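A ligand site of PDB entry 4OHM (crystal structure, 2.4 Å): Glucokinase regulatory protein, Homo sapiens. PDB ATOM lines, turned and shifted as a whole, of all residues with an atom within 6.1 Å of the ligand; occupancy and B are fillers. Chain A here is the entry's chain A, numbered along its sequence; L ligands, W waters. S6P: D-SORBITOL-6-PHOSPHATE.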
ATOM      1  N   GLY A 119      13.211   4.741  -5.597  1.00  0.00           N
ATOM      2  CA  GLY A 119      11.991   4.619  -4.795  1.00  0.00           C
ATOM      3  C   GLY A 119      11.502   3.198  -4.913  1.00  0.00           C
ATOM      4  O   GLY A 119      11.841   2.536  -5.924  1.00  0.00           O
ATOM      5  N   GLY A 120      10.769   2.713  -3.903  1.00  0.00           N
ATOM      6  CA  GLY A 120      10.097   1.426  -3.966  1.00  0.00           C
ATOM      7  C   GLY A 120      11.106   0.317  -4.232  1.00  0.00           C
ATOM      8  O   GLY A 120      12.205   0.288  -3.632  1.00  0.00           O
ATOM      9  N   THR A 121      10.785  -0.560  -5.180  1.00  0.00           N
ATOM     10  CA  THR A 121      11.673  -1.680  -5.463  1.00  0.00           C
ATOM     11  C   THR A 121      13.009  -1.297  -6.008  1.00  0.00           C
ATOM     12  O   THR A 121      13.963  -2.024  -5.819  1.00  0.00           O
ATOM     13  CB  THR A 121      11.025  -2.644  -6.401  1.00  0.00           C
ATOM     14  OG1 THR A 121       9.782  -3.003  -5.828  1.00  0.00           O
ATOM     15  CG2 THR A 121      11.862  -3.867  -6.583  1.00  0.00           C
ATOM     16  N   SER A 122      13.140  -0.129  -6.605  1.00  0.00           N
ATOM     17  CA  SER A 122      14.475   0.309  -7.023  1.00  0.00           C
ATOM     18  C   SER A 122      15.277   0.649  -5.821  1.00  0.00           C
ATOM     19  O   SER A 122      16.520   0.602  -5.844  1.00  0.00           O
ATOM     20  CB  SER A 122      14.372   1.598  -7.854  1.00  0.00           C
ATOM     21  OG  SER A 122      13.754   1.293  -9.075  1.00  0.00           O
ATOM     22  N   ARG A 124      14.757  -0.753  -2.812  1.00  0.00           N
ATOM     23  CA  ARG A 124      15.095  -2.013  -2.240  1.00  0.00           C
ATOM     24  C   ARG A 124      16.344  -2.611  -2.924  1.00  0.00           C
ATOM     25  O   ARG A 124      17.305  -3.033  -2.250  1.00  0.00           O
ATOM     26  CB  ARG A 124      13.930  -2.944  -2.382  1.00  0.00           C
ATOM     27  CG  ARG A 124      12.723  -2.580  -1.540  1.00  0.00           C
ATOM     28  CD  ARG A 124      11.689  -3.712  -1.553  1.00  0.00           C
ATOM     29  NE  ARG A 124      10.336  -3.254  -1.890  1.00  0.00           N
ATOM     30  CZ  ARG A 124       9.575  -2.488  -1.107  1.00  0.00           C
ATOM     31  NH1 ARG A 124      10.007  -2.077   0.075  1.00  0.00           N
ATOM     32  NH2 ARG A 124       8.383  -2.134  -1.505  1.00  0.00           N
ATOM     33  N   GLU A 162       4.238   3.497  -0.944  1.00  0.00           N
ATOM     34  CA  GLU A 162       4.213   3.903  -2.354  1.00  0.00           C
ATOM     35  C   GLU A 162       4.160   5.419  -2.572  1.00  0.00           C
ATOM     36  O   GLU A 162       4.593   5.899  -3.624  1.00  0.00           O
ATOM     37  CB  GLU A 162       3.029   3.272  -3.063  1.00  0.00           C
ATOM     38  CG  GLU A 162       3.185   1.799  -3.312  1.00  0.00           C
ATOM     39  CD  GLU A 162       4.207   1.514  -4.393  1.00  0.00           C
ATOM     40  OE1 GLU A 162       3.793   1.133  -5.521  1.00  0.00           O
ATOM     41  OE2 GLU A 162       5.418   1.672  -4.087  1.00  0.00           O
ATOM     42  N   GLU A 165       7.616   8.534  -3.147  1.00  0.00           N
ATOM     43  CA  GLU A 165       8.425   8.872  -4.338  1.00  0.00           C
ATOM     44  C   GLU A 165       8.121  10.199  -5.086  1.00  0.00           C
ATOM     45  O   GLU A 165       8.825  10.549  -6.057  1.00  0.00           O
ATOM     46  CB  GLU A 165       8.349   7.726  -5.347  1.00  0.00           C
ATOM     47  CG  GLU A 165       6.996   7.394  -5.936  1.00  0.00           C
ATOM     48  CD  GLU A 165       7.092   6.374  -7.077  1.00  0.00           C
ATOM     49  OE1 GLU A 165       7.173   5.189  -6.775  1.00  0.00           O
ATOM     50  OE2 GLU A 165       7.043   6.749  -8.276  1.00  0.00           O
ATOM     51  N   ILE A 190      18.081   5.226  -9.794  1.00  0.00           N
ATOM     52  CA  ILE A 190      17.420   4.095 -10.378  1.00  0.00           C
ATOM     53  C   ILE A 190      15.933   4.356 -10.419  1.00  0.00           C
ATOM     54  O   ILE A 190      15.294   4.476  -9.386  1.00  0.00           O
ATOM     55  CB  ILE A 190      17.688   2.817  -9.530  1.00  0.00           C
ATOM     56  CG1 ILE A 190      19.202   2.570  -9.413  1.00  0.00           C
ATOM     57  CG2 ILE A 190      16.923   1.617 -10.106  1.00  0.00           C
ATOM     58  CD1 ILE A 190      19.537   1.383  -8.514  1.00  0.00           C
ATOM     59  N   SER A 191      15.385   4.440 -11.622  1.00  0.00           N
ATOM     60  CA  SER A 191      13.943   4.530 -11.814  1.00  0.00           C
ATOM     61  C   SER A 191      13.631   3.813 -13.100  1.00  0.00           C
ATOM     62  O   SER A 191      14.020   4.265 -14.193  1.00  0.00           O
ATOM     63  CB  SER A 191      13.423   5.975 -11.898  1.00  0.00           C
ATOM     64  OG  SER A 191      12.011   5.996 -11.967  1.00  0.00           O
ATOM     65  N   VAL A 192      12.936   2.709 -12.948  1.00  0.00           N
ATOM     66  CA  VAL A 192      12.701   1.822 -13.993  1.00  0.00           C
ATOM     67  C   VAL A 192      11.969   2.486 -15.097  1.00  0.00           C
ATOM     68  O   VAL A 192      12.237   2.222 -16.270  1.00  0.00           O
ATOM     69  CB  VAL A 192      11.882   0.650 -13.505  1.00  0.00           C
ATOM     70  CG1 VAL A 192      11.376  -0.158 -14.690  1.00  0.00           C
ATOM     71  CG2 VAL A 192      12.744  -0.239 -12.617  1.00  0.00           C
ATOM     72  N   GLY A 193      11.020   3.320 -14.719  1.00  0.00           N
ATOM     73  CA  GLY A 193      10.175   3.951 -15.682  1.00  0.00           C
ATOM     74  C   GLY A 193      10.740   5.276 -16.127  1.00  0.00           C
ATOM     75  O   GLY A 193      10.103   5.951 -16.896  1.00  0.00           O
ATOM     76  N   LEU A 194      11.928   5.638 -15.655  1.00  0.00           N
ATOM     77  CA  LEU A 194      12.428   7.018 -15.761  1.00  0.00           C
ATOM     78  C   LEU A 194      11.246   7.927 -15.372  1.00  0.00           C
ATOM     79  O   LEU A 194      10.822   8.785 -16.132  1.00  0.00           O
ATOM     80  CB  LEU A 194      12.947   7.301 -17.148  1.00  0.00           C
ATOM     81  CG  LEU A 194      14.068   6.424 -17.694  1.00  0.00           C
ATOM     82  CD1 LEU A 194      14.576   7.006 -19.006  1.00  0.00           C
ATOM     83  CD2 LEU A 194      15.208   6.346 -16.697  1.00  0.00           C
ATOM     84  N   SER A 195      10.715   7.669 -14.175  1.00  0.00           N
ATOM     85  CA  SER A 195       9.503   8.205 -13.657  1.00  0.00           C
ATOM     86  C   SER A 195       9.618   8.974 -12.327  1.00  0.00           C
ATOM     87  O   SER A 195       8.927   9.958 -12.162  1.00  0.00           O
ATOM     88  CB  SER A 195       8.517   7.057 -13.430  1.00  0.00           C
ATOM     89  OG  SER A 195       7.466   7.447 -12.546  1.00  0.00           O
ATOM     90  N   ALA A 196      10.438   8.493 -11.379  1.00  0.00           N
ATOM     91  CA  ALA A 196      10.219   8.878  -9.992  1.00  0.00           C
ATOM     92  C   ALA A 196      10.769  10.276  -9.674  1.00  0.00           C
ATOM     93  O   ALA A 196      11.936  10.554  -9.923  1.00  0.00           O
ATOM     94  CB  ALA A 196      10.811   7.838  -9.055  1.00  0.00           C
ATOM     95  N   VAL A 199      14.069  10.589  -7.789  1.00  0.00           N
ATOM     96  CA  VAL A 199      15.345  10.503  -8.501  1.00  0.00           C
ATOM     97  C   VAL A 199      15.595  11.745  -9.352  1.00  0.00           C
ATOM     98  O   VAL A 199      16.722  12.268  -9.433  1.00  0.00           O
ATOM     99  CB  VAL A 199      15.351   9.260  -9.431  1.00  0.00           C
ATOM    100  CG1 VAL A 199      16.636   9.127 -10.230  1.00  0.00           C
ATOM    101  CG2 VAL A 199      15.079   7.980  -8.619  1.00  0.00           C
ATOM    102  N   GLY A 268       3.096  -2.780 -15.907  1.00  0.00           N
ATOM    103  CA  GLY A 268       3.521  -1.779 -15.001  1.00  0.00           C
ATOM    104  C   GLY A 268       4.002  -2.285 -13.664  1.00  0.00           C
ATOM    105  O   GLY A 268       4.229  -1.471 -12.737  1.00  0.00           O
ATOM    106  N   SER A 269       4.147  -3.604 -13.528  1.00  0.00           N
ATOM    107  CA  SER A 269       4.614  -4.186 -12.273  1.00  0.00           C
ATOM    108  C   SER A 269       6.121  -4.222 -12.328  1.00  0.00           C
ATOM    109  O   SER A 269       6.735  -5.275 -12.430  1.00  0.00           O
ATOM    110  CB  SER A 269       4.028  -5.568 -12.021  1.00  0.00           C
ATOM    111  OG  SER A 269       4.376  -5.965 -10.706  1.00  0.00           O
ATOM    112  N   SER A 270       6.735  -3.031 -12.298  1.00  0.00           N
ATOM    113  CA  SER A 270       8.159  -2.918 -12.486  1.00  0.00           C
ATOM    114  C   SER A 270       9.021  -3.513 -11.335  1.00  0.00           C
ATOM    115  O   SER A 270      10.283  -3.430 -11.369  1.00  0.00           O
ATOM    116  CB  SER A 270       8.522  -1.437 -12.713  1.00  0.00           C
ATOM    117  OG  SER A 270       8.330  -0.678 -11.555  1.00  0.00           O
ATOM    118  N   ARG A 271       8.381  -4.066 -10.303  1.00  0.00           N
ATOM    119  CA  ARG A 271       9.145  -4.743  -9.268  1.00  0.00           C
ATOM    120  C   ARG A 271       9.806  -6.006  -9.831  1.00  0.00           C
ATOM    121  O   ARG A 271      10.831  -6.439  -9.324  1.00  0.00           O
ATOM    122  CB  ARG A 271       8.273  -5.099  -8.065  1.00  0.00           C
ATOM    123  CG  ARG A 271       7.278  -6.222  -8.302  1.00  0.00           C
ATOM    124  CD  ARG A 271       6.349  -6.363  -7.099  1.00  0.00           C
ATOM    125  NE  ARG A 271       5.562  -7.602  -7.181  1.00  0.00           N
ATOM    126  CZ  ARG A 271       5.860  -8.721  -6.513  1.00  0.00           C
ATOM    127  NH1 ARG A 271       6.895  -8.761  -5.697  1.00  0.00           N
ATOM    128  NH2 ARG A 271       5.115  -9.803  -6.679  1.00  0.00           N
ATOM    129  N   MET A 272       9.198  -6.570 -10.862  1.00  0.00           N
ATOM    130  CA  MET A 272       9.605  -7.809 -11.473  1.00  0.00           C
ATOM    131  C   MET A 272      10.755  -7.672 -12.469  1.00  0.00           C
ATOM    132  O   MET A 272      11.906  -7.576 -12.064  1.00  0.00           O
ATOM    133  CB  MET A 272       8.380  -8.433 -12.151  1.00  0.00           C
ATOM    134  CG  MET A 272       7.264  -8.735 -11.165  1.00  0.00           C
ATOM    135  SD  MET A 272       5.845  -9.349 -12.065  1.00  0.00           S
ATOM    136  CE  MET A 272       6.245 -11.106 -11.863  1.00  0.00           C
ATOM    137  N   GLU A 360       5.836  -6.289  -1.001  1.00  0.00           N
ATOM    138  CA  GLU A 360       5.391  -5.817  -2.303  1.00  0.00           C
ATOM    139  C   GLU A 360       3.998  -6.314  -2.638  1.00  0.00           C
ATOM    140  O   GLU A 360       3.259  -5.645  -3.389  1.00  0.00           O
ATOM    141  CB  GLU A 360       6.426  -6.150  -3.371  1.00  0.00           C
ATOM    142  CG  GLU A 360       7.683  -5.324  -3.130  1.00  0.00           C
ATOM    143  CD  GLU A 360       8.898  -5.733  -3.946  1.00  0.00           C
ATOM    144  OE1 GLU A 360       8.834  -6.756  -4.677  1.00  0.00           O
ATOM    145  OE2 GLU A 360       9.928  -4.990  -3.837  1.00  0.00           O
ATOM    146  N   HIS A 363       0.815  -3.585  -1.764  1.00  0.00           N
ATOM    147  CA  HIS A 363       0.362  -2.630  -2.767  1.00  0.00           C
ATOM    148  C   HIS A 363       0.100  -3.295  -4.099  1.00  0.00           C
ATOM    149  O   HIS A 363      -0.853  -2.957  -4.784  1.00  0.00           O
ATOM    150  CB  HIS A 363       1.312  -1.455  -2.913  1.00  0.00           C
ATOM    151  CG  HIS A 363       2.742  -1.825  -3.129  1.00  0.00           C
ATOM    152  ND1 HIS A 363       3.719  -1.626  -2.181  1.00  0.00           N
ATOM    153  CD2 HIS A 363       3.373  -2.341  -4.210  1.00  0.00           C
ATOM    154  CE1 HIS A 363       4.892  -2.011  -2.650  1.00  0.00           C
ATOM    155  NE2 HIS A 363       4.702  -2.454  -3.879  1.00  0.00           N
ATOM    156  N   THR A 364       0.882  -4.308  -4.463  1.00  0.00           N
ATOM    157  CA  THR A 364       0.706  -4.859  -5.780  1.00  0.00           C
ATOM    158  C   THR A 364      -0.632  -5.573  -5.910  1.00  0.00           C
ATOM    159  O   THR A 364      -1.284  -5.465  -6.941  1.00  0.00           O
ATOM    160  CB  THR A 364       1.860  -5.770  -6.178  1.00  0.00           C
ATOM    161  OG1 THR A 364       3.078  -5.016  -6.166  1.00  0.00           O
ATOM    162  CG2 THR A 364       1.617  -6.313  -7.566  1.00  0.00           C
ATOM    163  N   ASN A 524       0.114   7.051  -5.302  1.00  0.00           N
ATOM    164  CA  ASN A 524       1.030   8.066  -5.810  1.00  0.00           C
ATOM    165  C   ASN A 524       0.517   8.486  -7.171  1.00  0.00           C
ATOM    166  O   ASN A 524      -0.471   7.913  -7.671  1.00  0.00           O
ATOM    167  CB  ASN A 524       2.524   7.601  -5.825  1.00  0.00           C
ATOM    168  CG  ASN A 524       2.781   6.344  -6.651  1.00  0.00           C
ATOM    169  OD1 ASN A 524       3.661   5.519  -6.339  1.00  0.00           O
ATOM    170  ND2 ASN A 524       2.096   6.214  -7.701  1.00  0.00           N
ATOM    171  N   LYS A 526       1.885   8.360 -10.255  1.00  0.00           N
ATOM    172  CA  LYS A 526       2.007   7.374 -11.325  1.00  0.00           C
ATOM    173  C   LYS A 526       0.854   6.362 -11.356  1.00  0.00           C
ATOM    174  O   LYS A 526       0.310   6.029 -12.394  1.00  0.00           O
ATOM    175  CB  LYS A 526       3.337   6.650 -11.210  1.00  0.00           C
ATOM    176  CG  LYS A 526       3.529   5.532 -12.223  1.00  0.00           C
ATOM    177  CD  LYS A 526       4.951   4.978 -12.117  1.00  0.00           C
ATOM    178  CE  LYS A 526       5.215   4.292 -10.775  1.00  0.00           C
ATOM    179  NZ  LYS A 526       6.544   3.665 -10.848  1.00  0.00           N
ATOM    180  N   ARG A 530      -1.959   5.583 -14.124  1.00  0.00           N
ATOM    181  CA  ARG A 530      -2.221   4.220 -14.570  1.00  0.00           C
ATOM    182  C   ARG A 530      -3.702   3.835 -14.417  1.00  0.00           C
ATOM    183  O   ARG A 530      -4.277   3.149 -15.284  1.00  0.00           O
ATOM    184  CB  ARG A 530      -1.319   3.231 -13.831  1.00  0.00           C
ATOM    185  CG  ARG A 530      -1.389   1.791 -14.348  1.00  0.00           C
ATOM    186  CD  ARG A 530      -0.410   0.883 -13.605  1.00  0.00           C
ATOM    187  NE  ARG A 530       0.982   1.345 -13.728  1.00  0.00           N
ATOM    188  CZ  ARG A 530       1.961   1.158 -12.834  1.00  0.00           C
ATOM    189  NH1 ARG A 530       1.718   0.519 -11.701  1.00  0.00           N
ATOM    190  NH2 ARG A 530       3.201   1.622 -13.063  1.00  0.00           N
HETATM  191  C1  S6P L   1       6.480  -1.545  -8.852  1.00  0.00           C
HETATM  192  C2  S6P L   1       6.697  -1.272  -7.391  1.00  0.00           C
HETATM  193  C3  S6P L   1       6.922   0.185  -7.205  1.00  0.00           C
HETATM  194  C4  S6P L   1       8.113   0.693  -7.961  1.00  0.00           C
HETATM  195  C5  S6P L   1       8.327   2.139  -7.563  1.00  0.00           C
HETATM  196  C6  S6P L   1       9.457   2.739  -8.373  1.00  0.00           C
HETATM  197  O1  S6P L   1       5.983  -2.876  -9.028  1.00  0.00           O
HETATM  198  O2  S6P L   1       5.486  -1.534  -6.682  1.00  0.00           O
HETATM  199  O3  S6P L   1       7.082   0.475  -5.820  1.00  0.00           O
HETATM  200  O4  S6P L   1       9.277  -0.069  -7.677  1.00  0.00           O
HETATM  201  O5  S6P L   1       7.124   2.913  -7.840  1.00  0.00           O
HETATM  202  O6  S6P L   1       9.161   2.693  -9.768  1.00  0.00           O
HETATM  203  P   S6P L   1      10.301   3.267 -10.714  1.00  0.00           P
HETATM  204  O1P S6P L   1       9.846   3.143 -12.096  1.00  0.00           O
HETATM  205  O2P S6P L   1      11.583   2.412 -10.326  1.00  0.00           O
HETATM  206  O3P S6P L   1      10.743   4.725 -10.353  1.00  0.00           O
HETATM  207  O   HOH W   1       4.395   2.817  -7.354  1.00  0.00           O
HETATM  208  O   HOH W   2       7.594  -2.076  -4.316  1.00  0.00           O
HETATM  209  O   HOH W   3       8.297   5.927 -10.361  1.00  0.00           O
HETATM  210  O   HOH W   4      10.436  -0.199 -10.033  1.00  0.00           O
HETATM  211  O   HOH W   5      12.779   5.313  -8.420  1.00  0.00           O
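Merely in contact with the ligand: Ala 196, Gly 119, Ser 269 and Gly 120. 15 residues have an atom within 4 Å of the ligand: Gly 119, Gly 120, Thr 121, Ser 122, Glu 162, Glu 165, Ser 191, Val 192, Gly 193, Ala 196, Ser 269, Ser 270, Arg 271, His 363 and Lys 526. The nearest printed residue that does not touch the ligand is Thr 364 (4.3 Å).
Water W4 bridges O4 of the ligand and OG of Ser 270. Water W3 lies within hydrogen-bond range of the side-chain carboxylate (OE2) of Glu 165 (2.6 Å), an oxygen (O3P) of the ligand (2.7 Å), the side-chain hydroxyl (OG) of Ser 195 (2.8 Å), the side-chain amino group (NZ) of Lys 526 (2.9 Å) and the backbone NH (N) of Ala 196 (3.5 Å). Water W1 lies within hydrogen-bond range of OE1 of Glu 162 (2.6 Å), O5 of the ligand (2.8 Å) and OD1 of Asn 524 (3.0 Å). Water W5 lies within hydrogen-bond range of O of Ile 190 (2.8 Å), O3P of the ligand (2.9 Å) and N of Gly 119 (2.9 Å). Water W2 lies within hydrogen-bond range of the side-chain hydroxyl of Thr 121 (2.8 Å), the guanidinium group of Arg 124 (2.9 Å), a ring nitrogen (NE2) of His 363 (2.9 Å) and an oxygen (O3) of the ligand (3.0 Å).
The side-chain hydroxyl of Ser 191 lies within hydrogen-bond range of the backbone NH of Ala 196. The backbone NH (N) of Ser 195 sits at hydrogen-bond distance from the side-chain hydroxyl (OG) of Ser 191, at 3.1 Å. The side-chain amide oxygen (OD1) of Asn 524 sits close to the backbone carbonyl oxygen (O) of Glu 162, 2.9 Å away. The side-chain hydroxyl of Thr 121 is in hydrogen-bond range of the side-chain carboxylate of Glu 360, at 2.8 Å. OE1 of Glu 360 is in salt-bridge range of NH1 of Arg 271, 3.0 Å away. N of Lys 526 sits close to ND2 of Asn 524 (3.3 Å).
The side-chain hydroxyl (OG) of Ser 191 lies within hydrogen-bond range of an oxygen (O3P) of the ligand, 2.4 Å away. An oxygen (O5) of the ligand is in hydrogen-bond range of the side-chain carboxylate of Glu 165 (2.5 Å). An oxygen (O3) of the ligand lies within hydrogen-bond range of the side-chain carboxylate of Glu 162, 2.7 Å away. The side-chain hydroxyl (OG) of Ser 122 is in hydrogen-bond range of an oxygen (O2P) of the ligand (2.7 Å). N of Gly 193 sits at hydrogen-bond distance from O1P of the ligand. N of Thr 121 lies within hydrogen-bond range of O4 of the ligand. An oxygen (O1) of the ligand sits at hydrogen-bond distance from the backbone NH of Arg 271 (3.0 Å). The backbone NH of Val 192 lies within hydrogen-bond range of an oxygen (O2P) of the ligand (3.0 Å). The side-chain amino group (NZ) of Lys 526 lies within salt-bridge range of an oxygen (O1P) of the ligand, 3.6 Å away. A ring nitrogen (NE2) of His 363 lies within hydrogen-bond range of an oxygen (O2) of the ligand, at 3.1 Å. O1 of the ligand lies within hydrogen-bond range of N of Ser 270, at 3.4 Å.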
